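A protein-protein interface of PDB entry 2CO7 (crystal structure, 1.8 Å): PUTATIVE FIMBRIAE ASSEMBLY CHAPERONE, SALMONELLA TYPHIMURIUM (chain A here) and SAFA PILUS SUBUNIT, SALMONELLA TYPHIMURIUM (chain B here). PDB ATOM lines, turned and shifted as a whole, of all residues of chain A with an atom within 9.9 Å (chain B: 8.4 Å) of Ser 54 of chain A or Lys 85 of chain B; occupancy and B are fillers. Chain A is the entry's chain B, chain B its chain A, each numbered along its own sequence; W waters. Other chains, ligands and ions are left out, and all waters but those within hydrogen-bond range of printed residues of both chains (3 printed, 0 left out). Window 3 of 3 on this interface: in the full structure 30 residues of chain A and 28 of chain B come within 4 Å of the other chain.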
ATOM      1  N   SER A  47      12.102   4.829 -32.182  1.00  0.00           N
ATOM      2  CA  SER A  47      12.632   5.860 -31.297  1.00  0.00           C
ATOM      3  C   SER A  47      13.123   5.227 -29.980  1.00  0.00           C
ATOM      4  O   SER A  47      12.723   4.133 -29.654  1.00  0.00           O
ATOM      5  CB  SER A  47      11.522   6.893 -30.999  1.00  0.00           C
ATOM      6  OG  SER A  47      10.380   6.220 -30.455  1.00  0.00           O
ATOM      7  N   VAL A  48      14.032   5.892 -29.267  1.00  0.00           N
ATOM      8  CA  VAL A  48      14.408   5.491 -27.879  1.00  0.00           C
ATOM      9  C   VAL A  48      14.013   6.604 -26.907  1.00  0.00           C
ATOM     10  O   VAL A  48      14.292   7.777 -27.164  1.00  0.00           O
ATOM     11  CB  VAL A  48      15.926   5.175 -27.751  1.00  0.00           C
ATOM     12  CG1 VAL A  48      16.266   4.705 -26.342  1.00  0.00           C
ATOM     13  CG2 VAL A  48      16.311   4.058 -28.728  1.00  0.00           C
ATOM     14  N   LYS A  49      13.335   6.255 -25.817  1.00  0.00           N
ATOM     15  CA  LYS A  49      12.966   7.261 -24.795  1.00  0.00           C
ATOM     16  C   LYS A  49      13.618   6.853 -23.481  1.00  0.00           C
ATOM     17  O   LYS A  49      13.963   5.678 -23.283  1.00  0.00           O
ATOM     18  CB  LYS A  49      11.454   7.334 -24.601  1.00  0.00           C
ATOM     19  CG  LYS A  49      10.655   7.609 -25.890  1.00  0.00           C
ATOM     20  CD  LYS A  49      11.142   8.866 -26.516  1.00  0.00           C
ATOM     21  CE  LYS A  49      10.750  10.084 -25.785  1.00  0.00           C
ATOM     22  NZ  LYS A  49      10.633  11.252 -26.718  1.00  0.00           N
ATOM     23  N   ALA A  50      13.750   7.816 -22.577  1.00  0.00           N
ATOM     24  CA  ALA A  50      14.364   7.533 -21.274  1.00  0.00           C
ATOM     25  C   ALA A  50      13.388   6.658 -20.463  1.00  0.00           C
ATOM     26  O   ALA A  50      12.250   6.374 -20.940  1.00  0.00           O
ATOM     27  CB  ALA A  50      14.638   8.843 -20.552  1.00  0.00           C
ATOM     28  N   ALA A  51      13.809   6.214 -19.270  1.00  0.00           N
ATOM     29  CA  ALA A  51      12.928   5.364 -18.417  1.00  0.00           C
ATOM     30  C   ALA A  51      11.531   5.958 -18.181  1.00  0.00           C
ATOM     31  O   ALA A  51      10.541   5.207 -18.053  1.00  0.00           O
ATOM     32  CB  ALA A  51      13.623   5.040 -17.060  1.00  0.00           C
ATOM     33  N   ASP A  52      11.417   7.294 -18.101  1.00  0.00           N
ATOM     34  CA  ASP A  52      10.110   7.952 -17.851  1.00  0.00           C
ATOM     35  C   ASP A  52       9.151   7.963 -19.056  1.00  0.00           C
ATOM     36  O   ASP A  52       8.054   8.571 -19.015  1.00  0.00           O
ATOM     37  CB  ASP A  52      10.320   9.398 -17.332  1.00  0.00           C
ATOM     38  CG  ASP A  52      11.011  10.293 -18.348  1.00  0.00           C
ATOM     39  OD1 ASP A  52      11.470  11.390 -17.960  1.00  0.00           O
ATOM     40  OD2 ASP A  52      11.101   9.917 -19.547  1.00  0.00           O
ATOM     41  N   LYS A  53       9.612   7.324 -20.131  1.00  0.00           N
ATOM     42  CA  LYS A  53       8.884   7.141 -21.406  1.00  0.00           C
ATOM     43  C   LYS A  53       8.663   8.424 -22.216  1.00  0.00           C
ATOM     44  O   LYS A  53       7.919   8.405 -23.195  1.00  0.00           O
ATOM     45  CB  LYS A  53       7.537   6.418 -21.145  1.00  0.00           C
ATOM     46  CG  LYS A  53       7.695   5.003 -20.548  1.00  0.00           C
ATOM     47  CD  LYS A  53       6.317   4.464 -20.133  1.00  0.00           C
ATOM     48  CE  LYS A  53       6.469   3.022 -19.607  1.00  0.00           C
ATOM     49  NZ  LYS A  53       5.182   2.477 -19.167  1.00  0.00           N
ATOM     50  N   SER A  54       9.335   9.509 -21.845  1.00  0.00           N
ATOM     51  CA  SER A  54       9.031  10.833 -22.378  1.00  0.00           C
ATOM     52  C   SER A  54      10.273  11.625 -22.717  1.00  0.00           C
ATOM     53  O   SER A  54      10.306  12.300 -23.728  1.00  0.00           O
ATOM     54  CB  SER A  54       8.203  11.629 -21.337  1.00  0.00           C
ATOM     55  OG  SER A  54       7.106  10.820 -20.857  1.00  0.00           O
ATOM     56  N   SER A  55      11.286  11.508 -21.864  1.00  0.00           N
ATOM     57  CA  SER A  55      12.496  12.299 -21.980  1.00  0.00           C
ATOM     58  C   SER A  55      13.383  11.620 -23.046  1.00  0.00           C
ATOM     59  O   SER A  55      13.259  10.409 -23.273  1.00  0.00           O
ATOM     60  CB  SER A  55      13.220  12.340 -20.628  1.00  0.00           C
ATOM     61  OG  SER A  55      12.576  13.177 -19.664  1.00  0.00           O
ATOM     62  N   PRO A  56      14.298  12.384 -23.666  1.00  0.00           N
ATOM     63  CA  PRO A  56      15.233  11.769 -24.616  1.00  0.00           C
ATOM     64  C   PRO A  56      16.254  10.849 -23.953  1.00  0.00           C
ATOM     65  O   PRO A  56      16.547  10.964 -22.740  1.00  0.00           O
ATOM     66  CB  PRO A  56      15.988  12.979 -25.223  1.00  0.00           C
ATOM     67  CG  PRO A  56      15.165  14.224 -24.812  1.00  0.00           C
ATOM     68  CD  PRO A  56      14.533  13.839 -23.497  1.00  0.00           C
ATOM     69  N   ALA A  57      16.800   9.940 -24.753  1.00  0.00           N
ATOM     70  CA  ALA A  57      17.842   9.015 -24.295  1.00  0.00           C
ATOM     71  C   ALA A  57      19.001   9.070 -25.284  1.00  0.00           C
ATOM     72  O   ALA A  57      18.783   9.394 -26.469  1.00  0.00           O
ATOM     73  CB  ALA A  57      17.294   7.592 -24.215  1.00  0.00           C
ATOM     74  N   LEU A  92      17.743   2.284 -17.533  1.00  0.00           N
ATOM     75  CA  LEU A  92      16.700   1.747 -18.386  1.00  0.00           C
ATOM     76  C   LEU A  92      16.252   2.803 -19.385  1.00  0.00           C
ATOM     77  O   LEU A  92      16.131   3.987 -19.033  1.00  0.00           O
ATOM     78  CB  LEU A  92      15.505   1.296 -17.535  1.00  0.00           C
ATOM     79  CG  LEU A  92      14.473   0.582 -18.429  1.00  0.00           C
ATOM     80  CD1 LEU A  92      13.962  -0.737 -17.819  1.00  0.00           C
ATOM     81  CD2 LEU A  92      13.354   1.512 -18.747  1.00  0.00           C
ATOM     82  N   GLN A  93      16.033   2.373 -20.620  1.00  0.00           N
ATOM     83  CA  GLN A  93      15.377   3.183 -21.656  1.00  0.00           C
ATOM     84  C   GLN A  93      14.251   2.312 -22.267  1.00  0.00           C
ATOM     85  O   GLN A  93      14.101   1.118 -21.931  1.00  0.00           O
ATOM     86  CB  GLN A  93      16.396   3.487 -22.788  1.00  0.00           C
ATOM     87  CG  GLN A  93      17.470   4.463 -22.546  1.00  0.00           C
ATOM     88  CD  GLN A  93      18.613   3.985 -21.663  1.00  0.00           C
ATOM     89  OE1 GLN A  93      19.261   4.793 -21.079  1.00  0.00           O
ATOM     90  NE2 GLN A  93      18.878   2.676 -21.613  1.00  0.00           N
ATOM     91  N   TRP A  94      13.501   2.888 -23.207  1.00  0.00           N
ATOM     92  CA  TRP A  94      12.514   2.153 -23.960  1.00  0.00           C
ATOM     93  C   TRP A  94      12.770   2.354 -25.443  1.00  0.00           C
ATOM     94  O   TRP A  94      12.900   3.487 -25.897  1.00  0.00           O
ATOM     95  CB  TRP A  94      11.121   2.694 -23.670  1.00  0.00           C
ATOM     96  CG  TRP A  94      10.680   2.448 -22.265  1.00  0.00           C
ATOM     97  CD1 TRP A  94      10.858   3.290 -21.171  1.00  0.00           C
ATOM     98  CD2 TRP A  94      10.042   1.276 -21.773  1.00  0.00           C
ATOM     99  NE1 TRP A  94      10.344   2.692 -20.037  1.00  0.00           N
ATOM    100  CE2 TRP A  94       9.849   1.458 -20.370  1.00  0.00           C
ATOM    101  CE3 TRP A  94       9.643   0.071 -22.366  1.00  0.00           C
ATOM    102  CZ2 TRP A  94       9.207   0.501 -19.566  1.00  0.00           C
ATOM    103  CZ3 TRP A  94       8.970  -0.888 -21.554  1.00  0.00           C
ATOM    104  CH2 TRP A  94       8.804  -0.665 -20.164  1.00  0.00           C
ATOM    105  N   CYS A  96      10.940   1.894 -28.914  1.00  0.00           N
ATOM    106  CA  CYS A  96       9.556   1.833 -29.354  1.00  0.00           C
ATOM    107  C   CYS A  96       9.500   1.789 -30.875  1.00  0.00           C
ATOM    108  O   CYS A  96      10.269   2.461 -31.559  1.00  0.00           O
ATOM    109  CB  CYS A  96       8.828   3.068 -28.886  1.00  0.00           C
ATOM    110  SG  CYS A  96       8.589   3.163 -27.097  1.00  0.00           S
ATOM    111  N   CYS A 125       6.730  -1.184 -27.407  1.00  0.00           N
ATOM    112  CA  CYS A 125       7.947  -0.707 -26.751  1.00  0.00           C
ATOM    113  C   CYS A 125       8.598  -1.801 -25.893  1.00  0.00           C
ATOM    114  O   CYS A 125       7.898  -2.491 -25.100  1.00  0.00           O
ATOM    115  CB  CYS A 125       7.632   0.540 -25.900  1.00  0.00           C
ATOM    116  SG  CYS A 125       6.909   1.936 -26.847  1.00  0.00           S
ATOM    117  N   SER B  52      -8.542  15.515 -22.888  1.00  0.00           N
ATOM    118  CA  SER B  52      -7.122  15.259 -22.660  1.00  0.00           C
ATOM    119  C   SER B  52      -6.661  13.863 -23.078  1.00  0.00           C
ATOM    120  O   SER B  52      -5.563  13.694 -23.603  1.00  0.00           O
ATOM    121  CB  SER B  52      -6.791  15.453 -21.180  1.00  0.00           C
ATOM    122  OG  SER B  52      -5.413  15.772 -21.036  1.00  0.00           O
ATOM    123  N   THR B  53      -7.511  12.869 -22.848  1.00  0.00           N
ATOM    124  CA  THR B  53      -7.084  11.481 -23.008  1.00  0.00           C
ATOM    125  C   THR B  53      -7.444  10.851 -24.345  1.00  0.00           C
ATOM    126  O   THR B  53      -7.065   9.701 -24.609  1.00  0.00           O
ATOM    127  CB  THR B  53      -7.665  10.601 -21.902  1.00  0.00           C
ATOM    128  OG1 THR B  53      -9.094  10.708 -21.932  1.00  0.00           O
ATOM    129  CG2 THR B  53      -7.148  11.042 -20.551  1.00  0.00           C
ATOM    130  N   SER B  82      -5.339   3.261 -14.981  1.00  0.00           N
ATOM    131  CA  SER B  82      -4.716   4.537 -14.641  1.00  0.00           C
ATOM    132  C   SER B  82      -4.760   5.454 -15.855  1.00  0.00           C
ATOM    133  O   SER B  82      -5.131   5.023 -16.954  1.00  0.00           O
ATOM    134  CB  SER B  82      -3.250   4.312 -14.241  1.00  0.00           C
ATOM    135  OG  SER B  82      -2.457   3.895 -15.329  1.00  0.00           O
ATOM    136  N   THR B  83      -4.408   6.716 -15.628  1.00  0.00           N
ATOM    137  CA  THR B  83      -4.121   7.639 -16.699  1.00  0.00           C
ATOM    138  C   THR B  83      -2.664   8.047 -16.545  1.00  0.00           C
ATOM    139  O   THR B  83      -2.262   8.538 -15.476  1.00  0.00           O
ATOM    140  CB  THR B  83      -4.998   8.890 -16.650  1.00  0.00           C
ATOM    141  OG1 THR B  83      -6.382   8.511 -16.748  1.00  0.00           O
ATOM    142  CG2 THR B  83      -4.631   9.848 -17.793  1.00  0.00           C
ATOM    143  N   GLU B  84      -1.911   7.895 -17.624  1.00  0.00           N
ATOM    144  CA  GLU B  84      -0.464   8.160 -17.620  1.00  0.00           C
ATOM    145  C   GLU B  84      -0.122   9.200 -18.653  1.00  0.00           C
ATOM    146  O   GLU B  84      -0.604   9.155 -19.796  1.00  0.00           O
ATOM    147  CB  GLU B  84       0.299   6.883 -17.974  1.00  0.00           C
ATOM    148  CG  GLU B  84       0.032   5.722 -17.057  1.00  0.00           C
ATOM    149  CD  GLU B  84       0.852   5.776 -15.802  1.00  0.00           C
ATOM    150  OE1 GLU B  84       0.454   5.148 -14.801  1.00  0.00           O
ATOM    151  OE2 GLU B  84       1.887   6.468 -15.808  1.00  0.00           O
ATOM    152  N   LYS B  85       0.773  10.098 -18.286  1.00  0.00           N
ATOM    153  CA  LYS B  85       1.344  10.998 -19.288  1.00  0.00           C
ATOM    154  C   LYS B  85       2.641  10.417 -19.878  1.00  0.00           C
ATOM    155  O   LYS B  85       3.680  10.381 -19.225  1.00  0.00           O
ATOM    156  CB  LYS B  85       1.572  12.401 -18.705  1.00  0.00           C
ATOM    157  CG  LYS B  85       2.030  13.400 -19.745  1.00  0.00           C
ATOM    158  CD  LYS B  85       1.886  14.852 -19.310  1.00  0.00           C
ATOM    159  CE  LYS B  85       0.508  15.370 -19.761  1.00  0.00           C
ATOM    160  NZ  LYS B  85      -0.093  16.335 -18.833  1.00  0.00           N
ATOM    161  N   TRP B  86       2.563  10.000 -21.133  1.00  0.00           N
ATOM    162  CA  TRP B  86       3.687   9.403 -21.824  1.00  0.00           C
ATOM    163  C   TRP B  86       3.963  10.234 -23.046  1.00  0.00           C
ATOM    164  O   TRP B  86       3.077  10.473 -23.888  1.00  0.00           O
ATOM    165  CB  TRP B  86       3.328   8.000 -22.280  1.00  0.00           C
ATOM    166  CG  TRP B  86       3.115   6.980 -21.214  1.00  0.00           C
ATOM    167  CD1 TRP B  86       3.753   6.879 -20.003  1.00  0.00           C
ATOM    168  CD2 TRP B  86       2.255   5.849 -21.316  1.00  0.00           C
ATOM    169  NE1 TRP B  86       3.297   5.746 -19.323  1.00  0.00           N
ATOM    170  CE2 TRP B  86       2.391   5.100 -20.124  1.00  0.00           C
ATOM    171  CE3 TRP B  86       1.365   5.401 -22.303  1.00  0.00           C
ATOM    172  CZ2 TRP B  86       1.678   3.921 -19.899  1.00  0.00           C
ATOM    173  CZ3 TRP B  86       0.648   4.228 -22.067  1.00  0.00           C
ATOM    174  CH2 TRP B  86       0.815   3.509 -20.878  1.00  0.00           C
ATOM    175  N   ASN B  87       5.222  10.656 -23.146  1.00  0.00           N
ATOM    176  CA  ASN B  87       5.719  11.468 -24.239  1.00  0.00           C
ATOM    177  C   ASN B  87       4.822  12.673 -24.545  1.00  0.00           C
ATOM    178  O   ASN B  87       4.578  12.974 -25.716  1.00  0.00           O
ATOM    179  CB  ASN B  87       5.962  10.600 -25.490  1.00  0.00           C
ATOM    180  CG  ASN B  87       6.939  11.214 -26.454  1.00  0.00           C
ATOM    181  OD1 ASN B  87       7.821  12.021 -26.078  1.00  0.00           O
ATOM    182  ND2 ASN B  87       6.800  10.842 -27.735  1.00  0.00           N
ATOM    183  N   GLY B  88       4.354  13.347 -23.488  1.00  0.00           N
ATOM    184  CA  GLY B  88       3.671  14.625 -23.597  1.00  0.00           C
ATOM    185  C   GLY B  88       2.158  14.526 -23.724  1.00  0.00           C
ATOM    186  O   GLY B  88       1.468  15.565 -23.794  1.00  0.00           O
ATOM    187  N   VAL B  89       1.658  13.290 -23.766  1.00  0.00           N
ATOM    188  CA  VAL B  89       0.240  13.003 -24.066  1.00  0.00           C
ATOM    189  C   VAL B  89      -0.353  12.093 -22.972  1.00  0.00           C
ATOM    190  O   VAL B  89       0.313  11.128 -22.550  1.00  0.00           O
ATOM    191  CB  VAL B  89       0.127  12.315 -25.491  1.00  0.00           C
ATOM    192  CG1 VAL B  89      -1.314  12.176 -25.910  1.00  0.00           C
ATOM    193  CG2 VAL B  89       0.878  13.119 -26.535  1.00  0.00           C
ATOM    194  N   ASN B  90      -1.589  12.386 -22.534  1.00  0.00           N
ATOM    195  CA  ASN B  90      -2.336  11.533 -21.574  1.00  0.00           C
ATOM    196  C   ASN B  90      -2.990  10.346 -22.256  1.00  0.00           C
ATOM    197  O   ASN B  90      -3.628  10.510 -23.289  1.00  0.00           O
ATOM    198  CB  ASN B  90      -3.458  12.327 -20.852  1.00  0.00           C
ATOM    199  CG  ASN B  90      -2.913  13.332 -19.857  1.00  0.00           C
ATOM    200  OD1 ASN B  90      -1.712  13.480 -19.734  1.00  0.00           O
ATOM    201  ND2 ASN B  90      -3.796  14.018 -19.137  1.00  0.00           N
ATOM    202  N   TRP B  91      -2.832   9.174 -21.647  1.00  0.00           N
ATOM    203  CA  TRP B  91      -3.393   7.906 -22.130  1.00  0.00           C
ATOM    204  C   TRP B  91      -4.088   7.207 -20.989  1.00  0.00           C
ATOM    205  O   TRP B  91      -3.540   7.111 -19.890  1.00  0.00           O
ATOM    206  CB  TRP B  91      -2.269   6.963 -22.557  1.00  0.00           C
ATOM    207  CG  TRP B  91      -1.485   7.352 -23.742  1.00  0.00           C
ATOM    208  CD1 TRP B  91      -0.452   8.255 -23.788  1.00  0.00           C
ATOM    209  CD2 TRP B  91      -1.589   6.791 -25.066  1.00  0.00           C
ATOM    210  NE1 TRP B  91       0.067   8.312 -25.058  1.00  0.00           N
ATOM    211  CE2 TRP B  91      -0.608   7.422 -25.859  1.00  0.00           C
ATOM    212  CE3 TRP B  91      -2.434   5.825 -25.659  1.00  0.00           C
ATOM    213  CZ2 TRP B  91      -0.437   7.129 -27.235  1.00  0.00           C
ATOM    214  CZ3 TRP B  91      -2.272   5.545 -27.033  1.00  0.00           C
ATOM    215  CH2 TRP B  91      -1.277   6.194 -27.792  1.00  0.00           C
ATOM    216  N   MET B  92      -5.293   6.695 -21.230  1.00  0.00           N
ATOM    217  CA  MET B  92      -5.913   5.798 -20.277  1.00  0.00           C
ATOM    218  C   MET B  92      -5.379   4.386 -20.532  1.00  0.00           C
ATOM    219  O   MET B  92      -5.256   3.965 -21.685  1.00  0.00           O
ATOM    220  CB  MET B  92      -7.435   5.871 -20.414  1.00  0.00           C
ATOM    221  CG  MET B  92      -7.971   7.280 -20.164  1.00  0.00           C
ATOM    222  SD  MET B  92      -9.761   7.373 -19.950  1.00  0.00           S
ATOM    223  CE  MET B  92      -9.999   6.459 -18.422  1.00  0.00           C
ATOM    224  N   THR B  93      -5.033   3.678 -19.463  1.00  0.00           N
ATOM    225  CA  THR B  93      -4.456   2.350 -19.612  1.00  0.00           C
ATOM    226  C   THR B  93      -5.484   1.312 -19.210  1.00  0.00           C
ATOM    227  O   THR B  93      -6.384   1.599 -18.393  1.00  0.00           O
ATOM    228  CB  THR B  93      -3.129   2.162 -18.802  1.00  0.00           C
ATOM    229  OG1 THR B  93      -3.425   2.078 -17.402  1.00  0.00           O
ATOM    230  CG2 THR B  93      -2.161   3.330 -19.030  1.00  0.00           C
ATOM    231  N   TYR B 125       3.820  -1.206 -23.475  1.00  0.00           N
ATOM    232  CA  TYR B 125       5.187  -1.279 -22.930  1.00  0.00           C
ATOM    233  C   TYR B 125       5.390  -2.654 -22.306  1.00  0.00           C
ATOM    234  O   TYR B 125       4.697  -3.028 -21.328  1.00  0.00           O
ATOM    235  CB  TYR B 125       5.324  -0.212 -21.857  1.00  0.00           C
ATOM    236  CG  TYR B 125       5.258   1.177 -22.444  1.00  0.00           C
ATOM    237  CD1 TYR B 125       4.035   1.841 -22.590  1.00  0.00           C
ATOM    238  CD2 TYR B 125       6.433   1.816 -22.877  1.00  0.00           C
ATOM    239  CE1 TYR B 125       3.990   3.147 -23.130  1.00  0.00           C
ATOM    240  CE2 TYR B 125       6.399   3.105 -23.405  1.00  0.00           C
ATOM    241  CZ  TYR B 125       5.162   3.755 -23.535  1.00  0.00           C
ATOM    242  OH  TYR B 125       5.128   5.037 -24.082  1.00  0.00           O
HETATM  243  O   HOH W   1       4.126   3.925 -17.043  1.00  0.00           O
HETATM  244  O   HOH W   2       5.538  13.526 -21.052  1.00  0.00           O
HETATM  245  O   HOH W   3       7.310   6.277 -24.756  1.00  0.00           O
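Of the 16 printed residues of chain A, 5 touch a printed residue of chain B.
Of the 15 printed residues of chain B, 4 touch a printed residue of chain A.
Printed residues of chain B that touch a printed residue of chain A: Lys 85, Trp 86, Asn 87 and Tyr 125.
Hydrophobic or aromatic side chains of chain B that line the printed part of chain A: Trp 86 and Tyr 125.
O of Ser 54 of chain A lies close to NZ of Lys 49 of chain A, at 3.2 Å.
OD1 of Asn 90 of chain B sits close to NZ of Lys 85 of chain B.
The backbone carbonyl oxygen of Ala 51 of chain A lies within hydrogen-bond range of the indole nitrogen of Trp 94 of chain A (3.2 Å).
The side-chain carboxylate (OD2) of Asp 52 of chain A lies within hydrogen-bond range of the backbone NH (N) of Ser 54 of chain A (2.9 Å).
The side-chain sulfur (SG) of Cys 125 of chain A is disulfide-bonded to the side-chain sulfur (SG) of Cys 96 of chain A.
N of Lys 49 of chain A is in hydrogen-bond range of O of Trp 94 of chain A (2.8 Å).
NE1 of Trp 86 of chain B touches CD of Lys 53 of chain A, at 3.4 Å.
O of Lys 53 of chain A touches N of Asn 87 of chain B, at 3.5 Å.
Tyr 125 of chain B touches Lys 53 of chain A.
Ser 54 of chain A touches Lys 85 of chain B (OG to O, 3.8 Å).
Trp 86 of chain B touches Ser 54 of chain A (CA to OG, 3.8 Å).
CE3 of Trp 94 of chain A touches CD2 of Tyr 125 of chain B, at 3.7 Å.
Cys 125 of chain A touches Tyr 125 of chain B (CB to CD2, 3.5 Å).
The side-chain amide oxygen (OD1) of Asn 87 of chain B is in hydrogen-bond range of the side-chain amino group (NZ) of Lys 49 of chain A, 3.0 Å away.
The backbone NH of Asn 87 of chain B sits at hydrogen-bond distance from the side-chain hydroxyl of Ser 54 of chain A, at 3.0 Å.
Printed residues of chain B within 4 Å of Lys 49 of chain A: Asn 87 (3.0 Å).
Of chain B, only Lys 85, Trp 86 and Asn 87 come within 4 Å of Ser 54 of chain A.
No residue of chain B comes within 4 Å of Ser 55 of chain A.
Of the printed residues of chain B, Trp 94 of chain A touches Tyr 125.
Lys 85 of chain B touches just one residue of chain A: Ser 54 (3.8 Å).
Of chain A, only Lys 49, Lys 53 and Ser 54 come within 4 Å of Asn 87 of chain B.
No residue of chain A comes within 4 Å of Gly 88 of chain B.
Val 89 of chain B touches none of the printed residues of chain A.
Asn 90 of chain B touches none of the printed residues of chain A.
Printed residues of chain A within 4 Å of Tyr 125 of chain B: Lys 53 (3.5 Å), Trp 94 (3.7 Å) and Cys 125 (3.5 Å).
The nearest residue of chain B that does not touch Ser 54 of chain A is Gly 88 of chain B (4.6 Å).
Water W3 bridges the side-chain hydroxyl of Tyr 125 of chain B and the backbone carbonyl oxygen of Lys 53 of chain A.
Water W2 bridges the backbone NH (N) of Gly 88 of chain B (2.7 Å) and the side-chain hydroxyl (OG) of Ser 54 of chain A (3.1 Å).
Water W1 lies within hydrogen-bond range of NZ of Lys 53 of chain A (2.8 Å) and NE1 of Trp 86 of chain B (3.0 Å).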
